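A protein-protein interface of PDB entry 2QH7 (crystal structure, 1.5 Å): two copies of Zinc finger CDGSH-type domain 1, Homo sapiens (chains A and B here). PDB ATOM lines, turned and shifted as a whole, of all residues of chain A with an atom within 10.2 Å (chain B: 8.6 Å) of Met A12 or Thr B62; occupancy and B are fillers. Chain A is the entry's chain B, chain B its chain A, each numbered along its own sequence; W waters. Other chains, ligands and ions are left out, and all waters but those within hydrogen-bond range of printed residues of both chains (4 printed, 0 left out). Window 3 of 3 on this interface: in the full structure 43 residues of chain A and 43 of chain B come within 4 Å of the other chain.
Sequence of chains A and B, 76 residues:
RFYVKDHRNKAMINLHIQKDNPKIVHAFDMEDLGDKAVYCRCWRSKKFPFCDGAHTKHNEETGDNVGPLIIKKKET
The side-chain amide oxygen of Asn B65 is in hydrogen-bond range of the side-chain amino group of Lys A19, at 2.9 Å. ND2 of Asn B65 is in hydrogen-bond range of O of Gln A18 (3.0 Å). The side-chain carboxylate (OD2) of Asp B64 is in hydrogen-bond range of the backbone NH (N) of Ile A13 (2.7 Å). The backbone NH (N) of Ile B13 is in hydrogen-bond range of the side-chain carboxylate (OD2) of Asp A64 (2.8 Å). N of Ile A24 sits at hydrogen-bond distance from O of Asn B65 (2.8 Å). The side-chain amide nitrogen (ND2) of Asn A14 sits at hydrogen-bond distance from the side-chain amide oxygen (OD1) of Asn B65 (2.9 Å). The side-chain sulfur (SD) of Met A12 lies close to the backbone carbonyl oxygen (O) of Gly B63. N of Asn A14 lies within hydrogen-bond range of OD2 of Asp B64 (3.1 Å). The side-chain carboxylate (OD1) of Asp B64 is in salt-bridge range of the side-chain amino group (NZ) of Lys A19, 3.0 Å away. The side-chain amide nitrogen (ND2) of Asn B65 lies within hydrogen-bond range of the backbone carbonyl oxygen (O) of Asn A21.
The side-chain carboxylate of Asp B64 is in hydrogen-bond range of a ring nitrogen (NE2) of His B58 (2.9 Å). The side-chain amino group (NZ) of Lys A19 is in hydrogen-bond range of the backbone carbonyl oxygen (O) of Asn A14. The backbone NH (N) of Asp A64 sits close to the side-chain hydroxyl (OG1) of Thr A62.
Among the printed residues, merely in contact across the chains: Cys A42 with Ile B13 (3.1 Å), Ile A13 with Cys B42 (3.2 Å), Thr A62 with Met B12 (3.3 Å), Thr A62 with Lys B10 (3.3 Å), Pro A22 with Asn B65 (3.4 Å), Ala A11 with Thr B62 (3.5 Å), Ile A13 with His B58 (3.5 Å), Trp A43 with Val B66 (3.5 Å), Asn A14 with Val B66 (3.6 Å), Ile A13 with Ile B13 (3.6 Å), Thr A62 with Ala B11 (3.6 Å), Ile A17 with Asn B65 (3.6 Å), Met A12 with Thr B62 (3.6 Å), Met A12 with Asp B64 (3.6 Å), His A58 with Ile B13 (3.7 Å), His A58 with Ala B11 (3.7 Å), Ala A11 with His B58 (3.7 Å), Asp A64 with Met B12 (3.7 Å) and Ile A24 with Val B66 (3.9 Å).
Ala A11 touches just these residues of chain B: His B58 and Thr B62. Printed residues of chain B within 4 Å of His A58: Ala B11 (3.7 Å) and Ile B13 (3.7 Å). Of the printed residues of chain B, Asp A64 touches Met B12 and Ile B13. Of the printed residues of chain A, Met B12 touches Thr A62 (3.3 Å) and Asp A64 (3.7 Å). Lys B57 touches none of the printed residues of chain A. Of chain A, only Ala A11 (3.7 Å) and Ile A13 (3.5 Å) come within 4 Å of His B58. Of chain A, only Ala A11 and Met A12 come within 4 Å of Thr B62. The nearest residue of chain B that does not touch Met A12 is His B58 (4.5 Å). The nearest residue of chain A that does not touch Thr B62 is Ile A13 (5.5 Å).
Printed residues of chain B that touch a printed residue of chain A: Lys B10, Ala B11, Met B12, Ile B13, Cys B42, His B58, Thr B62, Gly B63, Asp B64, Asn B65 and Val B66. Hydrophobic or aromatic side chains of chain B that line the printed part of chain A: Met B12, Ile B13, His B58 and Val B66. Among the printed residues, 29 pairs touch across the chains.
Met A12 touches Thr B62, and with the chains exchanged Thr A62 touches Met B12. Ile A13 touches Cys B42, and with the chains exchanged Cys A42 touches Ile B13. Ile A13 touches Asp B64, and with the chains exchanged Asp A64 touches Ile B13.
Water W1 bridges O of Ala B11 (2.5 Å) and NH2 of Arg A44 (3.0 Å). Water W4 lies within hydrogen-bond range of O of Lys B10 (2.6 Å) and O of Thr A62 (3.1 Å). Water W2 lies within hydrogen-bond range of O of Pro A22 (2.8 Å) and O of Asp B64 (3.4 Å).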
ATOM      1  N   ALA A  11     -30.541  17.917  33.927  1.00  0.00           N
ATOM      2  CA  ALA A  11     -30.953  17.591  32.533  1.00  0.00           C
ATOM      3  C   ALA A  11     -30.152  18.406  31.521  1.00  0.00           C
ATOM      4  O   ALA A  11     -30.098  19.633  31.600  1.00  0.00           O
ATOM      5  CB  ALA A  11     -32.438  17.845  32.339  1.00  0.00           C
ATOM      6  N   MET A  12     -29.539  17.719  30.563  1.00  0.00           N
ATOM      7  CA  MET A  12     -28.945  18.384  29.411  1.00  0.00           C
ATOM      8  C   MET A  12     -30.022  18.836  28.440  1.00  0.00           C
ATOM      9  O   MET A  12     -31.083  18.216  28.314  1.00  0.00           O
ATOM     10  CB  MET A  12     -27.979  17.455  28.685  1.00  0.00           C
ATOM     11  CG  MET A  12     -26.807  17.015  29.530  1.00  0.00           C
ATOM     12  SD  MET A  12     -25.488  16.312  28.532  1.00  0.00           S
ATOM     13  CE  MET A  12     -26.284  14.879  27.820  1.00  0.00           C
ATOM     14  N   ILE A  13     -29.724  19.926  27.758  1.00  0.00           N
ATOM     15  CA  ILE A  13     -30.557  20.440  26.683  1.00  0.00           C
ATOM     16  C   ILE A  13     -30.235  19.705  25.382  1.00  0.00           C
ATOM     17  O   ILE A  13     -31.126  19.153  24.738  1.00  0.00           O
ATOM     18  CB  ILE A  13     -30.353  21.961  26.541  1.00  0.00           C
ATOM     19  CG1 ILE A  13     -30.906  22.668  27.785  1.00  0.00           C
ATOM     20  CG2 ILE A  13     -31.000  22.490  25.280  1.00  0.00           C
ATOM     21  CD1 ILE A  13     -30.469  24.122  27.924  1.00  0.00           C
ATOM     22  N   ASN A  14     -28.962  19.687  25.006  1.00  0.00           N
ATOM     23  CA  ASN A  14     -28.503  18.930  23.845  1.00  0.00           C
ATOM     24  C   ASN A  14     -28.228  17.474  24.218  1.00  0.00           C
ATOM     25  O   ASN A  14     -27.474  17.175  25.145  1.00  0.00           O
ATOM     26  CB  ASN A  14     -27.287  19.605  23.203  1.00  0.00           C
ATOM     27  CG  ASN A  14     -26.704  18.805  22.059  1.00  0.00           C
ATOM     28  OD1 ASN A  14     -27.424  18.089  21.342  1.00  0.00           O
ATOM     29  ND2 ASN A  14     -25.373  18.884  21.905  1.00  0.00           N
ATOM     30  N   LEU A  15     -28.889  16.566  23.507  1.00  0.00           N
ATOM     31  CA  LEU A  15     -28.742  15.151  23.759  1.00  0.00           C
ATOM     32  C   LEU A  15     -27.717  14.457  22.867  1.00  0.00           C
ATOM     33  O   LEU A  15     -27.030  13.566  23.355  1.00  0.00           O
ATOM     34  CB  LEU A  15     -30.091  14.435  23.609  1.00  0.00           C
ATOM     35  CG  LEU A  15     -31.259  14.975  24.433  1.00  0.00           C
ATOM     36  CD1 LEU A  15     -32.468  14.073  24.264  1.00  0.00           C
ATOM     37  CD2 LEU A  15     -30.836  15.084  25.894  1.00  0.00           C
ATOM     38  N   HIS A  16     -27.617  14.864  21.594  1.00  0.00           N
ATOM     39  CA  HIS A  16     -26.903  14.080  20.580  1.00  0.00           C
ATOM     40  C   HIS A  16     -25.968  14.852  19.632  1.00  0.00           C
ATOM     41  O   HIS A  16     -25.155  14.247  18.963  1.00  0.00           O
ATOM     42  CB  HIS A  16     -27.919  13.260  19.762  1.00  0.00           C
ATOM     43  CG  HIS A  16     -28.527  13.999  18.607  1.00  0.00           C
ATOM     44  ND1 HIS A  16     -29.640  14.800  18.732  1.00  0.00           N
ATOM     45  CD2 HIS A  16     -28.188  14.033  17.296  1.00  0.00           C
ATOM     46  CE1 HIS A  16     -29.952  15.309  17.553  1.00  0.00           C
ATOM     47  NE2 HIS A  16     -29.088  14.855  16.663  1.00  0.00           N
ATOM     48  N   ILE A  17     -26.057  16.169  19.577  1.00  0.00           N
ATOM     49  CA  ILE A  17     -25.327  16.956  18.565  1.00  0.00           C
ATOM     50  C   ILE A  17     -23.858  17.216  18.974  1.00  0.00           C
ATOM     51  O   ILE A  17     -23.608  17.665  20.094  1.00  0.00           O
ATOM     52  CB  ILE A  17     -26.064  18.273  18.241  1.00  0.00           C
ATOM     53  CG1 ILE A  17     -27.443  17.965  17.632  1.00  0.00           C
ATOM     54  CG2 ILE A  17     -25.241  19.125  17.289  1.00  0.00           C
ATOM     55  CD1 ILE A  17     -28.407  19.102  17.750  1.00  0.00           C
ATOM     56  N   GLN A  18     -22.926  16.890  18.062  1.00  0.00           N
ATOM     57  CA  GLN A  18     -21.479  17.119  18.210  1.00  0.00           C
ATOM     58  C   GLN A  18     -20.976  17.025  19.641  1.00  0.00           C
ATOM     59  O   GLN A  18     -20.450  18.002  20.176  1.00  0.00           O
ATOM     60  CB  GLN A  18     -21.092  18.511  17.733  1.00  0.00           C
ATOM     61  CG  GLN A  18     -21.384  18.957  16.320  1.00  0.00           C
ATOM     62  CD  GLN A  18     -20.948  20.431  16.143  1.00  0.00           C
ATOM     63  OE1 GLN A  18     -19.773  20.790  16.391  1.00  0.00           O
ATOM     64  NE2 GLN A  18     -21.893  21.296  15.750  1.00  0.00           N
ATOM     65  N   LYS A  19     -21.136  15.877  20.283  1.00  0.00           N
ATOM     66  CA  LYS A  19     -20.743  15.757  21.694  1.00  0.00           C
ATOM     67  C   LYS A  19     -19.233  15.741  21.938  1.00  0.00           C
ATOM     68  O   LYS A  19     -18.797  15.821  23.082  1.00  0.00           O
ATOM     69  CB  LYS A  19     -21.413  14.557  22.357  1.00  0.00           C
ATOM     70  CG  LYS A  19     -22.914  14.739  22.650  1.00  0.00           C
ATOM     71  CD  LYS A  19     -23.196  15.978  23.514  1.00  0.00           C
ATOM     72  CE  LYS A  19     -24.604  16.064  24.044  1.00  0.00           C
ATOM     73  NZ  LYS A  19     -24.708  17.202  24.958  1.00  0.00           N
ATOM     74  N   ASN A  21     -17.472  18.155  20.770  1.00  0.00           N
ATOM     75  CA  ASN A  21     -17.227  19.591  20.865  1.00  0.00           C
ATOM     76  C   ASN A  21     -17.675  20.038  22.263  1.00  0.00           C
ATOM     77  O   ASN A  21     -18.855  19.898  22.589  1.00  0.00           O
ATOM     78  CB  ASN A  21     -18.029  20.303  19.763  1.00  0.00           C
ATOM     79  CG  ASN A  21     -17.836  21.794  19.754  1.00  0.00           C
ATOM     80  OD1 ASN A  21     -17.237  22.346  20.665  1.00  0.00           O
ATOM     81  ND2 ASN A  21     -18.334  22.459  18.716  1.00  0.00           N
ATOM     82  N   PRO A  22     -16.752  20.575  23.088  1.00  0.00           N
ATOM     83  CA  PRO A  22     -17.153  20.941  24.463  1.00  0.00           C
ATOM     84  C   PRO A  22     -18.099  22.149  24.596  1.00  0.00           C
ATOM     85  O   PRO A  22     -18.709  22.330  25.646  1.00  0.00           O
ATOM     86  CB  PRO A  22     -15.820  21.233  25.148  1.00  0.00           C
ATOM     87  CG  PRO A  22     -14.883  21.599  24.053  1.00  0.00           C
ATOM     88  CD  PRO A  22     -15.332  20.880  22.822  1.00  0.00           C
ATOM     89  N   ILE A  24     -20.721  24.185  21.747  1.00  0.00           N
ATOM     90  CA  ILE A  24     -21.140  24.341  20.375  1.00  0.00           C
ATOM     91  C   ILE A  24     -21.602  25.768  20.109  1.00  0.00           C
ATOM     92  O   ILE A  24     -22.628  26.198  20.628  1.00  0.00           O
ATOM     93  CB  ILE A  24     -22.262  23.358  19.997  1.00  0.00           C
ATOM     94  CG1 ILE A  24     -21.758  21.912  20.085  1.00  0.00           C
ATOM     95  CG2 ILE A  24     -22.751  23.627  18.561  1.00  0.00           C
ATOM     96  CD1 ILE A  24     -22.834  20.856  20.115  1.00  0.00           C
ATOM     97  N   CYS A  42     -33.749  24.477  19.869  1.00  0.00           N
ATOM     98  CA  CYS A  42     -34.207  23.310  20.634  1.00  0.00           C
ATOM     99  C   CYS A  42     -33.224  22.172  20.623  1.00  0.00           C
ATOM    100  O   CYS A  42     -33.420  21.220  21.329  1.00  0.00           O
ATOM    101  CB  CYS A  42     -35.588  22.776  20.143  1.00  0.00           C
ATOM    102  SG  CYS A  42     -35.612  21.905  18.570  1.00  0.00           S
ATOM    103  N   TRP A  43     -32.203  22.204  19.786  1.00  0.00           N
ATOM    104  CA  TRP A  43     -31.240  21.083  19.698  1.00  0.00           C
ATOM    105  C   TRP A  43     -31.797  19.715  19.309  1.00  0.00           C
ATOM    106  O   TRP A  43     -31.217  18.663  19.639  1.00  0.00           O
ATOM    107  CB  TRP A  43     -30.435  21.022  21.010  1.00  0.00           C
ATOM    108  CG  TRP A  43     -29.762  22.344  21.298  1.00  0.00           C
ATOM    109  CD1 TRP A  43     -30.328  23.403  21.878  1.00  0.00           C
ATOM    110  CD2 TRP A  43     -28.410  22.723  20.983  1.00  0.00           C
ATOM    111  NE1 TRP A  43     -29.425  24.422  21.982  1.00  0.00           N
ATOM    112  CE2 TRP A  43     -28.239  24.034  21.436  1.00  0.00           C
ATOM    113  CE3 TRP A  43     -27.328  22.062  20.376  1.00  0.00           C
ATOM    114  CZ2 TRP A  43     -27.039  24.736  21.282  1.00  0.00           C
ATOM    115  CZ3 TRP A  43     -26.126  22.745  20.248  1.00  0.00           C
ATOM    116  CH2 TRP A  43     -25.990  24.067  20.701  1.00  0.00           C
ATOM    117  N   ARG A  44     -32.916  19.719  18.572  1.00  0.00           N
ATOM    118  CA  ARG A  44     -33.573  18.532  18.129  1.00  0.00           C
ATOM    119  C   ARG A  44     -33.583  18.383  16.613  1.00  0.00           C
ATOM    120  O   ARG A  44     -33.806  17.267  16.117  1.00  0.00           O
ATOM    121  CB  ARG A  44     -35.026  18.462  18.633  1.00  0.00           C
ATOM    122  CG  ARG A  44     -35.165  18.443  20.152  1.00  0.00           C
ATOM    123  CD  ARG A  44     -34.499  17.270  20.735  1.00  0.00           C
ATOM    124  NE  ARG A  44     -34.630  17.201  22.186  1.00  0.00           N
ATOM    125  CZ  ARG A  44     -33.757  17.731  23.033  1.00  0.00           C
ATOM    126  NH1 ARG A  44     -32.670  18.332  22.587  1.00  0.00           N
ATOM    127  NH2 ARG A  44     -33.965  17.616  24.334  1.00  0.00           N
ATOM    128  N   HIS A  58     -40.972  18.179  20.126  1.00  0.00           N
ATOM    129  CA  HIS A  58     -40.379  18.443  21.457  1.00  0.00           C
ATOM    130  C   HIS A  58     -41.390  19.101  22.406  1.00  0.00           C
ATOM    131  O   HIS A  58     -41.593  18.652  23.543  1.00  0.00           O
ATOM    132  CB  HIS A  58     -39.130  19.307  21.366  1.00  0.00           C
ATOM    133  CG  HIS A  58     -38.702  19.858  22.690  1.00  0.00           C
ATOM    134  ND1 HIS A  58     -38.114  19.076  23.663  1.00  0.00           N
ATOM    135  CD2 HIS A  58     -38.876  21.076  23.244  1.00  0.00           C
ATOM    136  CE1 HIS A  58     -37.887  19.812  24.737  1.00  0.00           C
ATOM    137  NE2 HIS A  58     -38.333  21.034  24.506  1.00  0.00           N
ATOM    138  N   THR A  62     -43.011  17.307  25.771  1.00  0.00           N
ATOM    139  CA  THR A  62     -42.472  17.800  27.051  1.00  0.00           C
ATOM    140  C   THR A  62     -43.305  18.914  27.701  1.00  0.00           C
ATOM    141  O   THR A  62     -43.082  19.257  28.854  1.00  0.00           O
ATOM    142  CB  THR A  62     -41.034  18.327  26.893  1.00  0.00           C
ATOM    143  OG1 THR A  62     -41.010  19.455  26.013  1.00  0.00           O
ATOM    144  CG2 THR A  62     -40.130  17.261  26.343  1.00  0.00           C
ATOM    145  N   ASP A  64     -43.147  21.951  26.579  1.00  0.00           N
ATOM    146  CA  ASP A  64     -42.292  23.119  26.456  1.00  0.00           C
ATOM    147  C   ASP A  64     -42.893  24.101  25.443  1.00  0.00           C
ATOM    148  O   ASP A  64     -43.881  23.805  24.799  1.00  0.00           O
ATOM    149  CB  ASP A  64     -40.874  22.672  26.038  1.00  0.00           C
ATOM    150  CG  ASP A  64     -39.783  23.585  26.507  1.00  0.00           C
ATOM    151  OD1 ASP A  64     -40.057  24.670  27.052  1.00  0.00           O
ATOM    152  OD2 ASP A  64     -38.608  23.229  26.279  1.00  0.00           O
ATOM    153  N   LYS B  10     -38.287  13.862  27.597  1.00  0.00           N
ATOM    154  CA  LYS B  10     -39.241  14.127  28.707  1.00  0.00           C
ATOM    155  C   LYS B  10     -39.082  15.535  29.271  1.00  0.00           C
ATOM    156  O   LYS B  10     -40.074  16.228  29.508  1.00  0.00           O
ATOM    157  N   ALA B  11     -37.835  15.951  29.475  1.00  0.00           N
ATOM    158  CA  ALA B  11     -37.534  17.212  30.153  1.00  0.00           C
ATOM    159  C   ALA B  11     -37.672  18.432  29.244  1.00  0.00           C
ATOM    160  O   ALA B  11     -37.207  18.431  28.097  1.00  0.00           O
ATOM    161  CB  ALA B  11     -36.135  17.158  30.737  1.00  0.00           C
ATOM    162  N   MET B  12     -38.287  19.484  29.777  1.00  0.00           N
ATOM    163  CA  MET B  12     -38.321  20.751  29.086  1.00  0.00           C
ATOM    164  C   MET B  12     -36.917  21.335  29.023  1.00  0.00           C
ATOM    165  O   MET B  12     -36.105  21.126  29.908  1.00  0.00           O
ATOM    166  CB  MET B  12     -39.241  21.758  29.781  1.00  0.00           C
ATOM    167  CG  MET B  12     -40.697  21.393  29.768  1.00  0.00           C
ATOM    168  SD  MET B  12     -41.716  22.822  30.164  1.00  0.00           S
ATOM    169  CE  MET B  12     -41.035  23.392  31.710  1.00  0.00           C
ATOM    170  N   ILE B  13     -36.667  22.061  27.944  1.00  0.00           N
ATOM    171  CA  ILE B  13     -35.460  22.844  27.717  1.00  0.00           C
ATOM    172  C   ILE B  13     -35.573  24.229  28.359  1.00  0.00           C
ATOM    173  O   ILE B  13     -34.688  24.642  29.100  1.00  0.00           O
ATOM    174  CB  ILE B  13     -35.208  22.948  26.195  1.00  0.00           C
ATOM    175  CG1 ILE B  13     -34.770  21.578  25.656  1.00  0.00           C
ATOM    176  CG2 ILE B  13     -34.211  24.035  25.807  1.00  0.00           C
ATOM    177  CD1 ILE B  13     -34.720  21.544  24.130  1.00  0.00           C
ATOM    178  N   LEU B  15     -37.088  26.460  31.092  1.00  0.00           N
ATOM    179  CA  LEU B  15     -37.731  26.355  32.383  1.00  0.00           C
ATOM    180  C   LEU B  15     -38.644  27.551  32.704  1.00  0.00           C
ATOM    181  O   LEU B  15     -39.718  27.341  33.216  1.00  0.00           O
ATOM    182  CB  LEU B  15     -36.681  26.206  33.480  1.00  0.00           C
ATOM    183  CG  LEU B  15     -35.570  25.162  33.254  1.00  0.00           C
ATOM    184  CD1 LEU B  15     -34.576  25.149  34.397  1.00  0.00           C
ATOM    185  CD2 LEU B  15     -36.178  23.785  33.071  1.00  0.00           C
ATOM    186  N   CYS B  42     -29.641  28.373  24.846  1.00  0.00           N
ATOM    187  CA  CYS B  42     -29.760  27.565  26.052  1.00  0.00           C
ATOM    188  C   CYS B  42     -30.985  27.894  26.896  1.00  0.00           C
ATOM    189  O   CYS B  42     -31.240  27.199  27.864  1.00  0.00           O
ATOM    190  CB  CYS B  42     -28.496  27.705  26.932  1.00  0.00           C
ATOM    191  SG  CYS B  42     -28.245  29.315  27.772  1.00  0.00           S
ATOM    192  N   ARG B  44     -31.380  30.113  29.197  1.00  0.00           N
ATOM    193  CA  ARG B  44     -31.009  30.490  30.553  1.00  0.00           C
ATOM    194  C   ARG B  44     -30.602  31.943  30.675  1.00  0.00           C
ATOM    195  O   ARG B  44     -30.405  32.413  31.796  1.00  0.00           O
ATOM    196  CB  ARG B  44     -29.872  29.604  31.090  1.00  0.00           C
ATOM    197  CG  ARG B  44     -30.175  28.092  31.138  1.00  0.00           C
ATOM    198  CD  ARG B  44     -31.232  27.732  32.159  1.00  0.00           C
ATOM    199  NE  ARG B  44     -31.486  26.293  32.147  1.00  0.00           N
ATOM    200  CZ  ARG B  44     -32.358  25.687  31.343  1.00  0.00           C
ATOM    201  NH1 ARG B  44     -33.138  26.389  30.544  1.00  0.00           N
ATOM    202  NH2 ARG B  44     -32.501  24.370  31.399  1.00  0.00           N
ATOM    203  N   HIS B  55     -25.020  30.091  29.487  1.00  0.00           N
ATOM    204  CA  HIS B  55     -24.691  28.761  28.983  1.00  0.00           C
ATOM    205  C   HIS B  55     -23.523  28.079  29.690  1.00  0.00           C
ATOM    206  O   HIS B  55     -23.531  26.866  29.872  1.00  0.00           O
ATOM    207  CB  HIS B  55     -24.447  28.785  27.460  1.00  0.00           C
ATOM    208  CG  HIS B  55     -23.306  29.656  27.027  1.00  0.00           C
ATOM    209  ND1 HIS B  55     -23.470  30.968  26.628  1.00  0.00           N
ATOM    210  CD2 HIS B  55     -21.979  29.404  26.941  1.00  0.00           C
ATOM    211  CE1 HIS B  55     -22.291  31.487  26.337  1.00  0.00           C
ATOM    212  NE2 HIS B  55     -21.374  30.553  26.499  1.00  0.00           N
ATOM    213  N   THR B  56     -22.529  28.857  30.098  1.00  0.00           N
ATOM    214  CA  THR B  56     -21.337  28.301  30.734  1.00  0.00           C
ATOM    215  C   THR B  56     -21.717  27.610  32.046  1.00  0.00           C
ATOM    216  O   THR B  56     -21.298  26.489  32.294  1.00  0.00           O
ATOM    217  CB  THR B  56     -20.215  29.356  30.953  1.00  0.00           C
ATOM    218  OG1 THR B  56     -20.658  30.372  31.842  1.00  0.00           O
ATOM    219  CG2 THR B  56     -19.817  30.019  29.673  1.00  0.00           C
ATOM    220  N   LYS B  57     -22.540  28.266  32.862  1.00  0.00           N
ATOM    221  CA  LYS B  57     -23.053  27.667  34.101  1.00  0.00           C
ATOM    222  C   LYS B  57     -23.916  26.437  33.814  1.00  0.00           C
ATOM    223  O   LYS B  57     -23.793  25.414  34.486  1.00  0.00           O
ATOM    224  CB  LYS B  57     -23.863  28.700  34.907  1.00  0.00           C
ATOM    225  CG  LYS B  57     -24.461  28.192  36.215  1.00  0.00           C
ATOM    226  CD  LYS B  57     -25.258  29.285  36.937  1.00  0.00           C
ATOM    227  N   HIS B  58     -24.802  26.540  32.826  1.00  0.00           N
ATOM    228  CA  HIS B  58     -25.628  25.388  32.482  1.00  0.00           C
ATOM    229  C   HIS B  58     -24.759  24.170  32.130  1.00  0.00           C
ATOM    230  O   HIS B  58     -24.981  23.069  32.637  1.00  0.00           O
ATOM    231  CB  HIS B  58     -26.566  25.709  31.328  1.00  0.00           C
ATOM    232  CG  HIS B  58     -27.125  24.492  30.677  1.00  0.00           C
ATOM    233  ND1 HIS B  58     -28.179  23.781  31.204  1.00  0.00           N
ATOM    234  CD2 HIS B  58     -26.719  23.812  29.584  1.00  0.00           C
ATOM    235  CE1 HIS B  58     -28.427  22.735  30.435  1.00  0.00           C
ATOM    236  NE2 HIS B  58     -27.559  22.737  29.437  1.00  0.00           N
ATOM    237  N   ASN B  59     -23.785  24.391  31.242  1.00  0.00           N
ATOM    238  CA  ASN B  59     -22.862  23.340  30.826  1.00  0.00           C
ATOM    239  C   ASN B  59     -22.063  22.768  31.988  1.00  0.00           C
ATOM    240  O   ASN B  59     -21.837  21.565  32.060  1.00  0.00           O
ATOM    241  CB  ASN B  59     -21.885  23.868  29.769  1.00  0.00           C
ATOM    242  CG  ASN B  59     -22.532  24.104  28.416  1.00  0.00           C
ATOM    243  OD1 ASN B  59     -23.665  23.657  28.139  1.00  0.00           O
ATOM    244  ND2 ASN B  59     -21.814  24.816  27.543  1.00  0.00           N
ATOM    245  N   GLU B  60     -21.617  23.624  32.900  1.00  0.00           N
ATOM    246  CA  GLU B  60     -20.870  23.154  34.051  1.00  0.00           C
ATOM    247  C   GLU B  60     -21.773  22.337  34.974  1.00  0.00           C
ATOM    248  O   GLU B  60     -21.353  21.290  35.474  1.00  0.00           O
ATOM    249  CB  GLU B  60     -20.233  24.327  34.808  1.00  0.00           C
ATOM    250  CG  GLU B  60     -19.292  23.930  35.947  1.00  0.00           C
ATOM    251  CD  GLU B  60     -18.034  23.178  35.489  1.00  0.00           C
ATOM    252  OE1 GLU B  60     -17.487  23.499  34.408  1.00  0.00           O
ATOM    253  OE2 GLU B  60     -17.578  22.274  36.235  1.00  0.00           O
ATOM    254  N   GLU B  61     -23.003  22.812  35.179  1.00  0.00           N
ATOM    255  CA  GLU B  61     -23.964  22.160  36.080  1.00  0.00           C
ATOM    256  C   GLU B  61     -24.451  20.797  35.575  1.00  0.00           C
ATOM    257  O   GLU B  61     -24.706  19.904  36.380  1.00  0.00           O
ATOM    258  CB  GLU B  61     -25.179  23.081  36.346  1.00  0.00           C
ATOM    259  CG  GLU B  61     -24.934  24.179  37.413  1.00  0.00           C
ATOM    260  CD  GLU B  61     -26.065  25.224  37.520  1.00  0.00           C
ATOM    261  OE1 GLU B  61     -27.022  25.185  36.720  1.00  0.00           O
ATOM    262  OE2 GLU B  61     -25.988  26.099  38.409  1.00  0.00           O
ATOM    263  N   THR B  62     -24.583  20.650  34.256  1.00  0.00           N
ATOM    264  CA  THR B  62     -25.231  19.480  33.642  1.00  0.00           C
ATOM    265  C   THR B  62     -24.313  18.588  32.814  1.00  0.00           C
ATOM    266  O   THR B  62     -24.709  17.489  32.451  1.00  0.00           O
ATOM    267  CB  THR B  62     -26.412  19.913  32.741  1.00  0.00           C
ATOM    268  OG1 THR B  62     -25.947  20.707  31.634  1.00  0.00           O
ATOM    269  CG2 THR B  62     -27.414  20.717  33.557  1.00  0.00           C
ATOM    270  N   GLY B  63     -23.104  19.051  32.502  1.00  0.00           N
ATOM    271  CA  GLY B  63     -22.221  18.327  31.593  1.00  0.00           C
ATOM    272  C   GLY B  63     -22.567  18.502  30.122  1.00  0.00           C
ATOM    273  O   GLY B  63     -22.066  17.764  29.275  1.00  0.00           O
ATOM    274  N   ASP B  64     -23.390  19.508  29.816  1.00  0.00           N
ATOM    275  CA  ASP B  64     -23.829  19.793  28.463  1.00  0.00           C
ATOM    276  C   ASP B  64     -22.745  20.604  27.732  1.00  0.00           C
ATOM    277  O   ASP B  64     -21.707  20.958  28.317  1.00  0.00           O
ATOM    278  CB  ASP B  64     -25.179  20.532  28.514  1.00  0.00           C
ATOM    279  CG  ASP B  64     -26.059  20.319  27.275  1.00  0.00           C
ATOM    280  OD1 ASP B  64     -25.621  19.701  26.280  1.00  0.00           O
ATOM    281  OD2 ASP B  64     -27.201  20.817  27.284  1.00  0.00           O
ATOM    282  N   ASN B  65     -23.003  20.876  26.451  1.00  0.00           N
ATOM    283  CA  ASN B  65     -22.049  21.496  25.532  1.00  0.00           C
ATOM    284  C   ASN B  65     -22.723  22.492  24.582  1.00  0.00           C
ATOM    285  O   ASN B  65     -22.350  22.599  23.417  1.00  0.00           O
ATOM    286  CB  ASN B  65     -21.315  20.409  24.746  1.00  0.00           C
ATOM    287  CG  ASN B  65     -22.197  19.683  23.728  1.00  0.00           C
ATOM    288  OD1 ASN B  65     -23.416  19.600  23.870  1.00  0.00           O
ATOM    289  ND2 ASN B  65     -21.568  19.146  22.689  1.00  0.00           N
ATOM    290  N   VAL B  66     -23.725  23.204  25.082  1.00  0.00           N
ATOM    291  CA  VAL B  66     -24.457  24.146  24.271  1.00  0.00           C
ATOM    292  C   VAL B  66     -23.796  25.520  24.302  1.00  0.00           C
ATOM    293  O   VAL B  66     -23.094  25.857  25.233  1.00  0.00           O
ATOM    294  CB  VAL B  66     -25.960  24.243  24.685  1.00  0.00           C
ATOM    295  CG1 VAL B  66     -26.669  22.906  24.386  1.00  0.00           C
ATOM    296  CG2 VAL B  66     -26.127  24.671  26.158  1.00  0.00           C
HETATM  297  O   HOH W   1     -35.757  16.986  26.647  1.00  0.00           O
HETATM  298  O   HOH W   2     -18.497  20.303  27.507  1.00  0.00           O
HETATM  299  O   HOH W   3     -22.392  16.900  26.820  1.00  0.00           O
HETATM  300  O   HOH W   4     -41.798  17.436  30.998  1.00  0.00           O
